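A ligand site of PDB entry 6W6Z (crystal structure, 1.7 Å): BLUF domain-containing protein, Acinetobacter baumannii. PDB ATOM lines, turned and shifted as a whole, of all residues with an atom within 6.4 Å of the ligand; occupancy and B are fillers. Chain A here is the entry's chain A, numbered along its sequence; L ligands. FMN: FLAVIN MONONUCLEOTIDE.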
ATOM      1  N   TYR A   7       0.053  15.244  13.486  1.00  0.00           N
ATOM      2  CA  TYR A   7       0.338  13.802  13.387  1.00  0.00           C
ATOM      3  C   TYR A   7       1.750  13.557  13.862  1.00  0.00           C
ATOM      4  O   TYR A   7       2.607  14.451  13.949  1.00  0.00           O
ATOM      5  CB  TYR A   7       0.079  13.304  11.957  1.00  0.00           C
ATOM      6  CG  TYR A   7       1.188  13.687  11.027  1.00  0.00           C
ATOM      7  CD1 TYR A   7       2.324  12.901  10.921  1.00  0.00           C
ATOM      8  CD2 TYR A   7       1.171  14.910  10.353  1.00  0.00           C
ATOM      9  CE1 TYR A   7       3.393  13.289  10.125  1.00  0.00           C
ATOM     10  CE2 TYR A   7       2.213  15.290   9.527  1.00  0.00           C
ATOM     11  CZ  TYR A   7       3.344  14.480   9.425  1.00  0.00           C
ATOM     12  OH  TYR A   7       4.405  14.888   8.682  1.00  0.00           O
ATOM     13  N   SER A   9       4.969  10.444  13.311  1.00  0.00           N
ATOM     14  CA  SER A   9       5.430   9.392  12.360  1.00  0.00           C
ATOM     15  C   SER A   9       6.800   8.866  12.812  1.00  0.00           C
ATOM     16  O   SER A   9       7.481   9.544  13.598  1.00  0.00           O
ATOM     17  CB  SER A   9       5.519   9.896  10.941  1.00  0.00           C
ATOM     18  OG  SER A   9       6.554  10.852  10.833  1.00  0.00           O
ATOM     19  N   ILE A  25      13.364  17.877   3.266  1.00  0.00           N
ATOM     20  CA  ILE A  25      11.972  18.052   3.786  1.00  0.00           C
ATOM     21  C   ILE A  25      11.690  19.546   4.041  1.00  0.00           C
ATOM     22  O   ILE A  25      10.653  20.048   3.592  1.00  0.00           O
ATOM     23  CB  ILE A  25      11.763  17.197   5.032  1.00  0.00           C
ATOM     24  CG1 ILE A  25      11.787  15.693   4.687  1.00  0.00           C
ATOM     25  CG2 ILE A  25      10.503  17.591   5.756  1.00  0.00           C
ATOM     26  CD1 ILE A  25      11.904  14.791   5.896  1.00  0.00           C
ATOM     27  N   GLU A  28      11.485  21.633   0.775  1.00  0.00           N
ATOM     28  CA  GLU A  28      10.198  21.347   0.054  1.00  0.00           C
ATOM     29  C   GLU A  28       9.042  22.020   0.820  1.00  0.00           C
ATOM     30  O   GLU A  28       8.217  22.723   0.178  1.00  0.00           O
ATOM     31  CB  GLU A  28       9.942  19.858  -0.056  1.00  0.00           C
ATOM     32  CG  GLU A  28      10.955  19.118  -0.936  1.00  0.00           C
ATOM     33  CD  GLU A  28      10.924  17.617  -0.720  1.00  0.00           C
ATOM     34  OE1 GLU A  28       9.836  17.112  -0.408  1.00  0.00           O
ATOM     35  OE2 GLU A  28      11.985  16.951  -0.836  1.00  0.00           O
ATOM     36  N   ALA A  29       8.965  21.773   2.128  1.00  0.00           N
ATOM     37  CA  ALA A  29       7.831  22.253   2.982  1.00  0.00           C
ATOM     38  C   ALA A  29       7.746  23.778   2.882  1.00  0.00           C
ATOM     39  O   ALA A  29       6.682  24.335   2.659  1.00  0.00           O
ATOM     40  CB  ALA A  29       8.041  21.826   4.416  1.00  0.00           C
ATOM     41  N   ARG A  30       8.861  24.451   3.073  1.00  0.00           N
ATOM     42  CA  ARG A  30       8.830  25.926   3.177  1.00  0.00           C
ATOM     43  C   ARG A  30       8.370  26.565   1.860  1.00  0.00           C
ATOM     44  O   ARG A  30       7.675  27.598   1.926  1.00  0.00           O
ATOM     45  CB  ARG A  30      10.189  26.414   3.680  1.00  0.00           C
ATOM     46  CG  ARG A  30      10.333  26.231   5.180  1.00  0.00           C
ATOM     47  CD  ARG A  30      11.757  26.245   5.688  1.00  0.00           C
ATOM     48  NE  ARG A  30      11.771  26.021   7.107  1.00  0.00           N
ATOM     49  CZ  ARG A  30      12.868  25.855   7.866  1.00  0.00           C
ATOM     50  NH1 ARG A  30      14.080  25.917   7.310  1.00  0.00           N
ATOM     51  NH2 ARG A  30      12.752  25.678   9.164  1.00  0.00           N
ATOM     52  N   ASP A  31       8.831  26.048   0.723  1.00  0.00           N
ATOM     53  CA  ASP A  31       8.446  26.529  -0.635  1.00  0.00           C
ATOM     54  C   ASP A  31       6.971  26.247  -0.872  1.00  0.00           C
ATOM     55  O   ASP A  31       6.255  27.209  -1.198  1.00  0.00           O
ATOM     56  CB  ASP A  31       9.264  25.861  -1.742  1.00  0.00           C
ATOM     57  N   PHE A  32       6.509  24.996  -0.700  1.00  0.00           N
ATOM     58  CA  PHE A  32       5.105  24.583  -1.005  1.00  0.00           C
ATOM     59  C   PHE A  32       4.145  25.326  -0.071  1.00  0.00           C
ATOM     60  O   PHE A  32       3.092  25.813  -0.511  1.00  0.00           O
ATOM     61  CB  PHE A  32       4.877  23.070  -0.947  1.00  0.00           C
ATOM     62  N   ASN A  33       4.508  25.397   1.211  1.00  0.00           N
ATOM     63  CA  ASN A  33       3.599  25.933   2.259  1.00  0.00           C
ATOM     64  C   ASN A  33       3.401  27.431   2.026  1.00  0.00           C
ATOM     65  O   ASN A  33       2.262  27.902   2.170  1.00  0.00           O
ATOM     66  CB  ASN A  33       4.163  25.647   3.647  1.00  0.00           C
ATOM     67  CG  ASN A  33       4.013  24.175   3.963  1.00  0.00           C
ATOM     68  OD1 ASN A  33       3.570  23.387   3.125  1.00  0.00           O
ATOM     69  ND2 ASN A  33       4.384  23.795   5.168  1.00  0.00           N
ATOM     70  N   ILE A  38       0.070  27.758   3.972  1.00  0.00           N
ATOM     71  CA  ILE A  38       0.138  26.790   5.090  1.00  0.00           C
ATOM     72  C   ILE A  38       1.295  27.238   5.970  1.00  0.00           C
ATOM     73  O   ILE A  38       2.320  27.704   5.429  1.00  0.00           O
ATOM     74  CB  ILE A  38       0.259  25.359   4.555  1.00  0.00           C
ATOM     75  CG1 ILE A  38      -1.073  24.948   3.908  1.00  0.00           C
ATOM     76  CG2 ILE A  38       0.664  24.410   5.659  1.00  0.00           C
ATOM     77  CD1 ILE A  38      -0.995  23.682   3.118  1.00  0.00           C
ATOM     78  N   LEU A  42       7.569  21.409  12.516  1.00  0.00           N
ATOM     79  CA  LEU A  42       8.095  20.034  12.357  1.00  0.00           C
ATOM     80  C   LEU A  42       9.059  19.848  13.494  1.00  0.00           C
ATOM     81  O   LEU A  42       9.984  20.635  13.573  1.00  0.00           O
ATOM     82  CB  LEU A  42       8.783  19.842  11.008  1.00  0.00           C
ATOM     83  CG  LEU A  42       9.248  18.407  10.719  1.00  0.00           C
ATOM     84  CD1 LEU A  42       8.065  17.448  10.664  1.00  0.00           C
ATOM     85  CD2 LEU A  42      10.064  18.312   9.447  1.00  0.00           C
ATOM     86  N   PHE A  49       9.033  11.947  13.926  1.00  0.00           N
ATOM     87  CA  PHE A  49       8.535  13.318  13.653  1.00  0.00           C
ATOM     88  C   PHE A  49       7.237  13.586  14.386  1.00  0.00           C
ATOM     89  O   PHE A  49       6.400  12.726  14.627  1.00  0.00           O
ATOM     90  CB  PHE A  49       8.300  13.497  12.161  1.00  0.00           C
ATOM     91  CG  PHE A  49       9.491  13.367  11.274  1.00  0.00           C
ATOM     92  CD1 PHE A  49      10.395  14.431  11.155  1.00  0.00           C
ATOM     93  CD2 PHE A  49       9.693  12.226  10.503  1.00  0.00           C
ATOM     94  CE1 PHE A  49      11.458  14.347  10.263  1.00  0.00           C
ATOM     95  CE2 PHE A  49      10.791  12.134   9.659  1.00  0.00           C
ATOM     96  CZ  PHE A  49      11.668  13.206   9.528  1.00  0.00           C
ATOM     97  N   GLN A  51       4.362  16.693  13.406  1.00  0.00           N
ATOM     98  CA  GLN A  51       4.114  17.894  12.594  1.00  0.00           C
ATOM     99  C   GLN A  51       2.745  18.460  12.896  1.00  0.00           C
ATOM    100  O   GLN A  51       1.765  17.700  13.068  1.00  0.00           O
ATOM    101  CB  GLN A  51       4.293  17.595  11.113  1.00  0.00           C
ATOM    102  CG  GLN A  51       4.332  18.860  10.289  1.00  0.00           C
ATOM    103  CD  GLN A  51       4.616  18.621   8.825  1.00  0.00           C
ATOM    104  OE1 GLN A  51       4.155  17.632   8.245  1.00  0.00           O
ATOM    105  NE2 GLN A  51       5.416  19.503   8.236  1.00  0.00           N
ATOM    106  N   LEU A  53       0.196  21.244  10.893  1.00  0.00           N
ATOM    107  CA  LEU A  53      -0.109  22.045   9.691  1.00  0.00           C
ATOM    108  C   LEU A  53      -1.287  22.954  10.007  1.00  0.00           C
ATOM    109  O   LEU A  53      -2.296  22.453  10.557  1.00  0.00           O
ATOM    110  CB  LEU A  53      -0.464  21.113   8.527  1.00  0.00           C
ATOM    111  CG  LEU A  53       0.579  20.035   8.171  1.00  0.00           C
ATOM    112  CD1 LEU A  53       0.016  19.071   7.151  1.00  0.00           C
ATOM    113  CD2 LEU A  53       1.846  20.688   7.653  1.00  0.00           C
ATOM    114  N   LEU A  63      -2.541  18.225   1.446  1.00  0.00           N
ATOM    115  CA  LEU A  63      -1.102  18.181   1.786  1.00  0.00           C
ATOM    116  C   LEU A  63      -0.861  16.963   2.673  1.00  0.00           C
ATOM    117  O   LEU A  63       0.026  16.194   2.348  1.00  0.00           O
ATOM    118  CB  LEU A  63      -0.650  19.464   2.483  1.00  0.00           C
ATOM    119  CG  LEU A  63       0.758  19.426   3.080  1.00  0.00           C
ATOM    120  CD1 LEU A  63       1.807  19.083   2.025  1.00  0.00           C
ATOM    121  CD2 LEU A  63       1.127  20.739   3.729  1.00  0.00           C
ATOM    122  N   LYS A  66      -0.661  13.707   0.713  1.00  0.00           N
ATOM    123  CA  LYS A  66       0.666  13.659   0.051  1.00  0.00           C
ATOM    124  C   LYS A  66       1.749  13.245   1.051  1.00  0.00           C
ATOM    125  O   LYS A  66       2.515  12.345   0.722  1.00  0.00           O
ATOM    126  CB  LYS A  66       1.004  15.007  -0.601  1.00  0.00           C
ATOM    127  CG  LYS A  66       0.039  15.414  -1.698  1.00  0.00           C
ATOM    128  CD  LYS A  66       0.542  16.434  -2.746  1.00  0.00           C
ATOM    129  CE  LYS A  66       1.523  17.463  -2.235  1.00  0.00           C
ATOM    130  NZ  LYS A  66       2.917  16.954  -2.301  1.00  0.00           N
ATOM    131  N   ILE A  67       1.755  13.843   2.244  1.00  0.00           N
ATOM    132  CA  ILE A  67       2.823  13.571   3.255  1.00  0.00           C
ATOM    133  C   ILE A  67       2.715  12.093   3.655  1.00  0.00           C
ATOM    134  O   ILE A  67       3.779  11.429   3.902  1.00  0.00           O
ATOM    135  CB  ILE A  67       2.722  14.506   4.462  1.00  0.00           C
ATOM    136  CG1 ILE A  67       3.078  15.945   4.104  1.00  0.00           C
ATOM    137  CG2 ILE A  67       3.532  13.981   5.623  1.00  0.00           C
ATOM    138  CD1 ILE A  67       2.642  16.978   5.162  1.00  0.00           C
ATOM    139  N   GLN A  68       1.488  11.565   3.752  1.00  0.00           N
ATOM    140  CA  GLN A  68       1.318  10.162   4.203  1.00  0.00           C
ATOM    141  C   GLN A  68       2.077   9.206   3.299  1.00  0.00           C
ATOM    142  O   GLN A  68       2.376   8.146   3.773  1.00  0.00           O
ATOM    143  CB  GLN A  68      -0.139   9.719   4.184  1.00  0.00           C
ATOM    144  CG  GLN A  68      -0.981  10.247   5.310  1.00  0.00           C
ATOM    145  CD  GLN A  68      -2.424   9.940   4.958  1.00  0.00           C
ATOM    146  OE1 GLN A  68      -2.764   8.820   4.590  1.00  0.00           O
ATOM    147  NE2 GLN A  68      -3.287  10.950   4.995  1.00  0.00           N
ATOM    148  N   LYS A  69       2.271   9.542   2.010  1.00  0.00           N
ATOM    149  CA  LYS A  69       2.928   8.661   1.002  1.00  0.00           C
ATOM    150  C   LYS A  69       4.454   8.850   1.001  1.00  0.00           C
ATOM    151  O   LYS A  69       5.143   8.083   0.305  1.00  0.00           O
ATOM    152  CB  LYS A  69       2.334   8.944  -0.388  1.00  0.00           C
ATOM    153  CG  LYS A  69       0.830   8.810  -0.427  1.00  0.00           C
ATOM    154  CD  LYS A  69       0.227   9.117  -1.750  1.00  0.00           C
ATOM    155  CE  LYS A  69      -1.203   9.587  -1.599  1.00  0.00           C
ATOM    156  NZ  LYS A  69      -1.945   9.467  -2.872  1.00  0.00           N
ATOM    157  N   ASP A  70       4.993   9.824   1.743  1.00  0.00           N
ATOM    158  CA  ASP A  70       6.420  10.205   1.607  1.00  0.00           C
ATOM    159  C   ASP A  70       7.272   9.001   2.024  1.00  0.00           C
ATOM    160  O   ASP A  70       7.001   8.482   3.113  1.00  0.00           O
ATOM    161  CB  ASP A  70       6.713  11.485   2.387  1.00  0.00           C
ATOM    162  CG  ASP A  70       8.046  12.117   2.030  1.00  0.00           C
ATOM    163  OD1 ASP A  70       9.101  11.455   2.254  1.00  0.00           O
ATOM    164  OD2 ASP A  70       8.018  13.262   1.560  1.00  0.00           O
ATOM    165  N   GLN A  71       8.274   8.631   1.217  1.00  0.00           N
ATOM    166  CA  GLN A  71       9.240   7.516   1.479  1.00  0.00           C
ATOM    167  C   GLN A  71      10.033   7.716   2.804  1.00  0.00           C
ATOM    168  O   GLN A  71      10.566   6.706   3.394  1.00  0.00           O
ATOM    169  CB  GLN A  71      10.229   7.454   0.315  1.00  0.00           C
ATOM    170  CG  GLN A  71      11.206   6.288   0.393  1.00  0.00           C
ATOM    171  CD  GLN A  71      12.494   6.590   1.133  1.00  0.00           C
ATOM    172  OE1 GLN A  71      12.913   7.735   1.241  1.00  0.00           O
ATOM    173  NE2 GLN A  71      13.137   5.534   1.611  1.00  0.00           N
ATOM    174  N   ARG A  72      10.149   8.949   3.253  1.00  0.00           N
ATOM    175  CA  ARG A  72      11.114   9.335   4.356  1.00  0.00           C
ATOM    176  C   ARG A  72      10.544   9.053   5.749  1.00  0.00           C
ATOM    177  O   ARG A  72      11.303   9.146   6.789  1.00  0.00           O
ATOM    178  CB  ARG A  72      11.526  10.790   4.144  1.00  0.00           C
ATOM    179  CG  ARG A  72      12.446  10.922   2.934  1.00  0.00           C
ATOM    180  CD  ARG A  72      12.667  12.315   2.444  1.00  0.00           C
ATOM    181  NE  ARG A  72      11.467  12.927   1.908  1.00  0.00           N
ATOM    182  CZ  ARG A  72      11.460  14.111   1.337  1.00  0.00           C
ATOM    183  NH1 ARG A  72      12.604  14.776   1.212  1.00  0.00           N
ATOM    184  NH2 ARG A  72      10.341  14.644   0.882  1.00  0.00           N
ATOM    185  N   HIS A  73       9.272   8.687   5.858  1.00  0.00           N
ATOM    186  CA  HIS A  73       8.667   8.287   7.150  1.00  0.00           C
ATOM    187  C   HIS A  73       7.570   7.248   6.894  1.00  0.00           C
ATOM    188  O   HIS A  73       7.270   6.999   5.683  1.00  0.00           O
ATOM    189  CB  HIS A  73       8.187   9.523   7.930  1.00  0.00           C
ATOM    190  CG  HIS A  73       7.026  10.220   7.306  1.00  0.00           C
ATOM    191  ND1 HIS A  73       6.319  11.154   7.987  1.00  0.00           N
ATOM    192  CD2 HIS A  73       6.463  10.132   6.077  1.00  0.00           C
ATOM    193  CE1 HIS A  73       5.342  11.615   7.218  1.00  0.00           C
ATOM    194  NE2 HIS A  73       5.404  11.023   6.022  1.00  0.00           N
ATOM    195  N   SER A  93       6.357  29.247   7.657  1.00  0.00           N
ATOM    196  CA  SER A  93       5.924  28.323   6.572  1.00  0.00           C
ATOM    197  C   SER A  93       6.107  26.869   7.056  1.00  0.00           C
ATOM    198  O   SER A  93       5.136  26.080   6.959  1.00  0.00           O
ATOM    199  CB  SER A  93       6.635  28.617   5.297  1.00  0.00           C
ATOM    200  OG  SER A  93       6.138  29.871   4.817  1.00  0.00           O
ATOM    201  N   MET A  94       7.243  26.605   7.665  1.00  0.00           N
ATOM    202  CA  MET A  94       7.461  25.367   8.467  1.00  0.00           C
ATOM    203  C   MET A  94       8.615  25.557   9.438  1.00  0.00           C
ATOM    204  O   MET A  94       9.785  25.453   9.008  1.00  0.00           O
ATOM    205  CB  MET A  94       7.782  24.177   7.564  1.00  0.00           C
ATOM    206  CG  MET A  94       7.793  22.863   8.330  1.00  0.00           C
ATOM    207  SD  MET A  94       6.386  22.554   9.446  1.00  0.00           S
ATOM    208  CE  MET A  94       5.033  22.804   8.301  1.00  0.00           C
HETATM  209  N1  FMN L   1       5.777  19.011   2.032  1.00  0.00           N
HETATM  210  C2  FMN L   1       5.194  20.213   2.085  1.00  0.00           C
HETATM  211  O2  FMN L   1       4.886  20.755   0.974  1.00  0.00           O
HETATM  212  N3  FMN L   1       4.812  20.780   3.240  1.00  0.00           N
HETATM  213  C4  FMN L   1       5.062  20.233   4.435  1.00  0.00           C
HETATM  214  O4  FMN L   1       4.755  20.765   5.501  1.00  0.00           O
HETATM  215  C4A FMN L   1       5.760  18.945   4.466  1.00  0.00           C
HETATM  216  N5  FMN L   1       6.069  18.329   5.593  1.00  0.00           N
HETATM  217  C5A FMN L   1       6.653  17.108   5.507  1.00  0.00           C
HETATM  218  C6  FMN L   1       6.976  16.478   6.689  1.00  0.00           C
HETATM  219  C7  FMN L   1       7.540  15.214   6.690  1.00  0.00           C
HETATM  220  C7M FMN L   1       7.881  14.603   8.007  1.00  0.00           C
HETATM  221  C8  FMN L   1       7.957  14.581   5.429  1.00  0.00           C
HETATM  222  C8M FMN L   1       8.636  13.212   5.483  1.00  0.00           C
HETATM  223  C9  FMN L   1       7.624  15.215   4.238  1.00  0.00           C
HETATM  224  C9A FMN L   1       7.032  16.471   4.251  1.00  0.00           C
HETATM  225  N10 FMN L   1       6.743  17.164   3.087  1.00  0.00           N
HETATM  226  C10 FMN L   1       6.087  18.376   3.170  1.00  0.00           C
HETATM  227  C1' FMN L   1       7.088  16.641   1.718  1.00  0.00           C
HETATM  228  C2' FMN L   1       5.992  15.945   0.953  1.00  0.00           C
HETATM  229  O2' FMN L   1       5.787  14.645   1.519  1.00  0.00           O
HETATM  230  C3' FMN L   1       6.442  15.820  -0.522  1.00  0.00           C
HETATM  231  O3' FMN L   1       7.789  15.348  -0.628  1.00  0.00           O
HETATM  232  C4' FMN L   1       6.465  17.144  -1.266  1.00  0.00           C
HETATM  233  O4' FMN L   1       5.181  17.794  -1.135  1.00  0.00           O
HETATM  234  C5' FMN L   1       6.763  16.924  -2.769  1.00  0.00           C
HETATM  235  O5' FMN L   1       5.750  16.144  -3.436  1.00  0.00           O
HETATM  236  P   FMN L   1       5.761  15.837  -5.060  1.00  0.00           P
HETATM  237  O1P FMN L   1       6.473  14.495  -5.139  1.00  0.00           O
HETATM  238  O2P FMN L   1       4.279  15.821  -5.383  1.00  0.00           O
HETATM  239  O3P FMN L   1       6.552  16.952  -5.728  1.00  0.00           O
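OD2 of Asp 70 sits at hydrogen-bond distance from O2' of the ligand (2.6 Å). NZ of Lys 66 is in salt-bridge range of O2P of the ligand. The side-chain carboxylate of Glu 28 is in hydrogen-bond range of an oxygen (O3') of the ligand (2.7 Å). The side-chain amide oxygen of Asn 33 sits at hydrogen-bond distance from a nitrogen (N3) of the ligand, at 2.9 Å. The side-chain amide nitrogen of Gln 51 is in hydrogen-bond range of a nitrogen (N5) of the ligand (3.0 Å). The guanidinium group (NH2) of Arg 72 is in hydrogen-bond range of an oxygen (O3') of the ligand, 3.0 Å away.
OD2 of Asp 70 is in salt-bridge range of NH2 of Arg 72, at 2.8 Å. The guanidinium group (NH2) of Arg 72 is in salt-bridge range of the side-chain carboxylate (OE1) of Glu 28, 2.8 Å away. The backbone carbonyl oxygen (O) of Ala 29 lies close to the side-chain amide oxygen (OD1) of Asn 33 (3.3 Å). The side-chain amide nitrogen (ND2) of Asn 33 sits at hydrogen-bond distance from the backbone carbonyl oxygen (O) of Ser 93 (3.0 Å). The side-chain amide nitrogen (NE2) of Gln 51 lies close to the side-chain sulfur (SD) of Met 94 (3.4 Å). OE1 of Gln 51 sits at hydrogen-bond distance from OH of Tyr 7 (2.8 Å). The backbone NH of Leu 42 is in hydrogen-bond range of the side-chain sulfur of Met 94 (3.5 Å). O of Ile 67 sits at hydrogen-bond distance from NE2 of His 73, at 2.7 Å.
Residues that only touch the ligand: Phe 32 (3.0 Å), Ala 29 (3.4 Å), Met 94 (3.5 Å), Tyr 7 (3.6 Å), Leu 63 (3.6 Å), Ile 67 (3.6 Å), Leu 53 (3.6 Å), Ile 25 (3.7 Å), His 73 (3.8 Å), Phe 49 (3.8 Å) and Leu 42 (3.9 Å). Hydrophobic or aromatic side chains that line the ligand: Ile 25, Ala 29, Phe 32, Leu 42, Phe 49, Leu 53, Leu 63, Ile 67, His 73 and Met 94. Within 4 Å of the ligand: Tyr 7, Ile 25, Glu 28, Ala 29, Phe 32, Asn 33, Leu 42, Phe 49, Gln 51, Leu 53, Leu 63, Lys 66, Ile 67, Asp 70, Arg 72, His 73 and Met 94. The nearest printed residue that does not touch the ligand is Ser 9 (4.9 Å).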
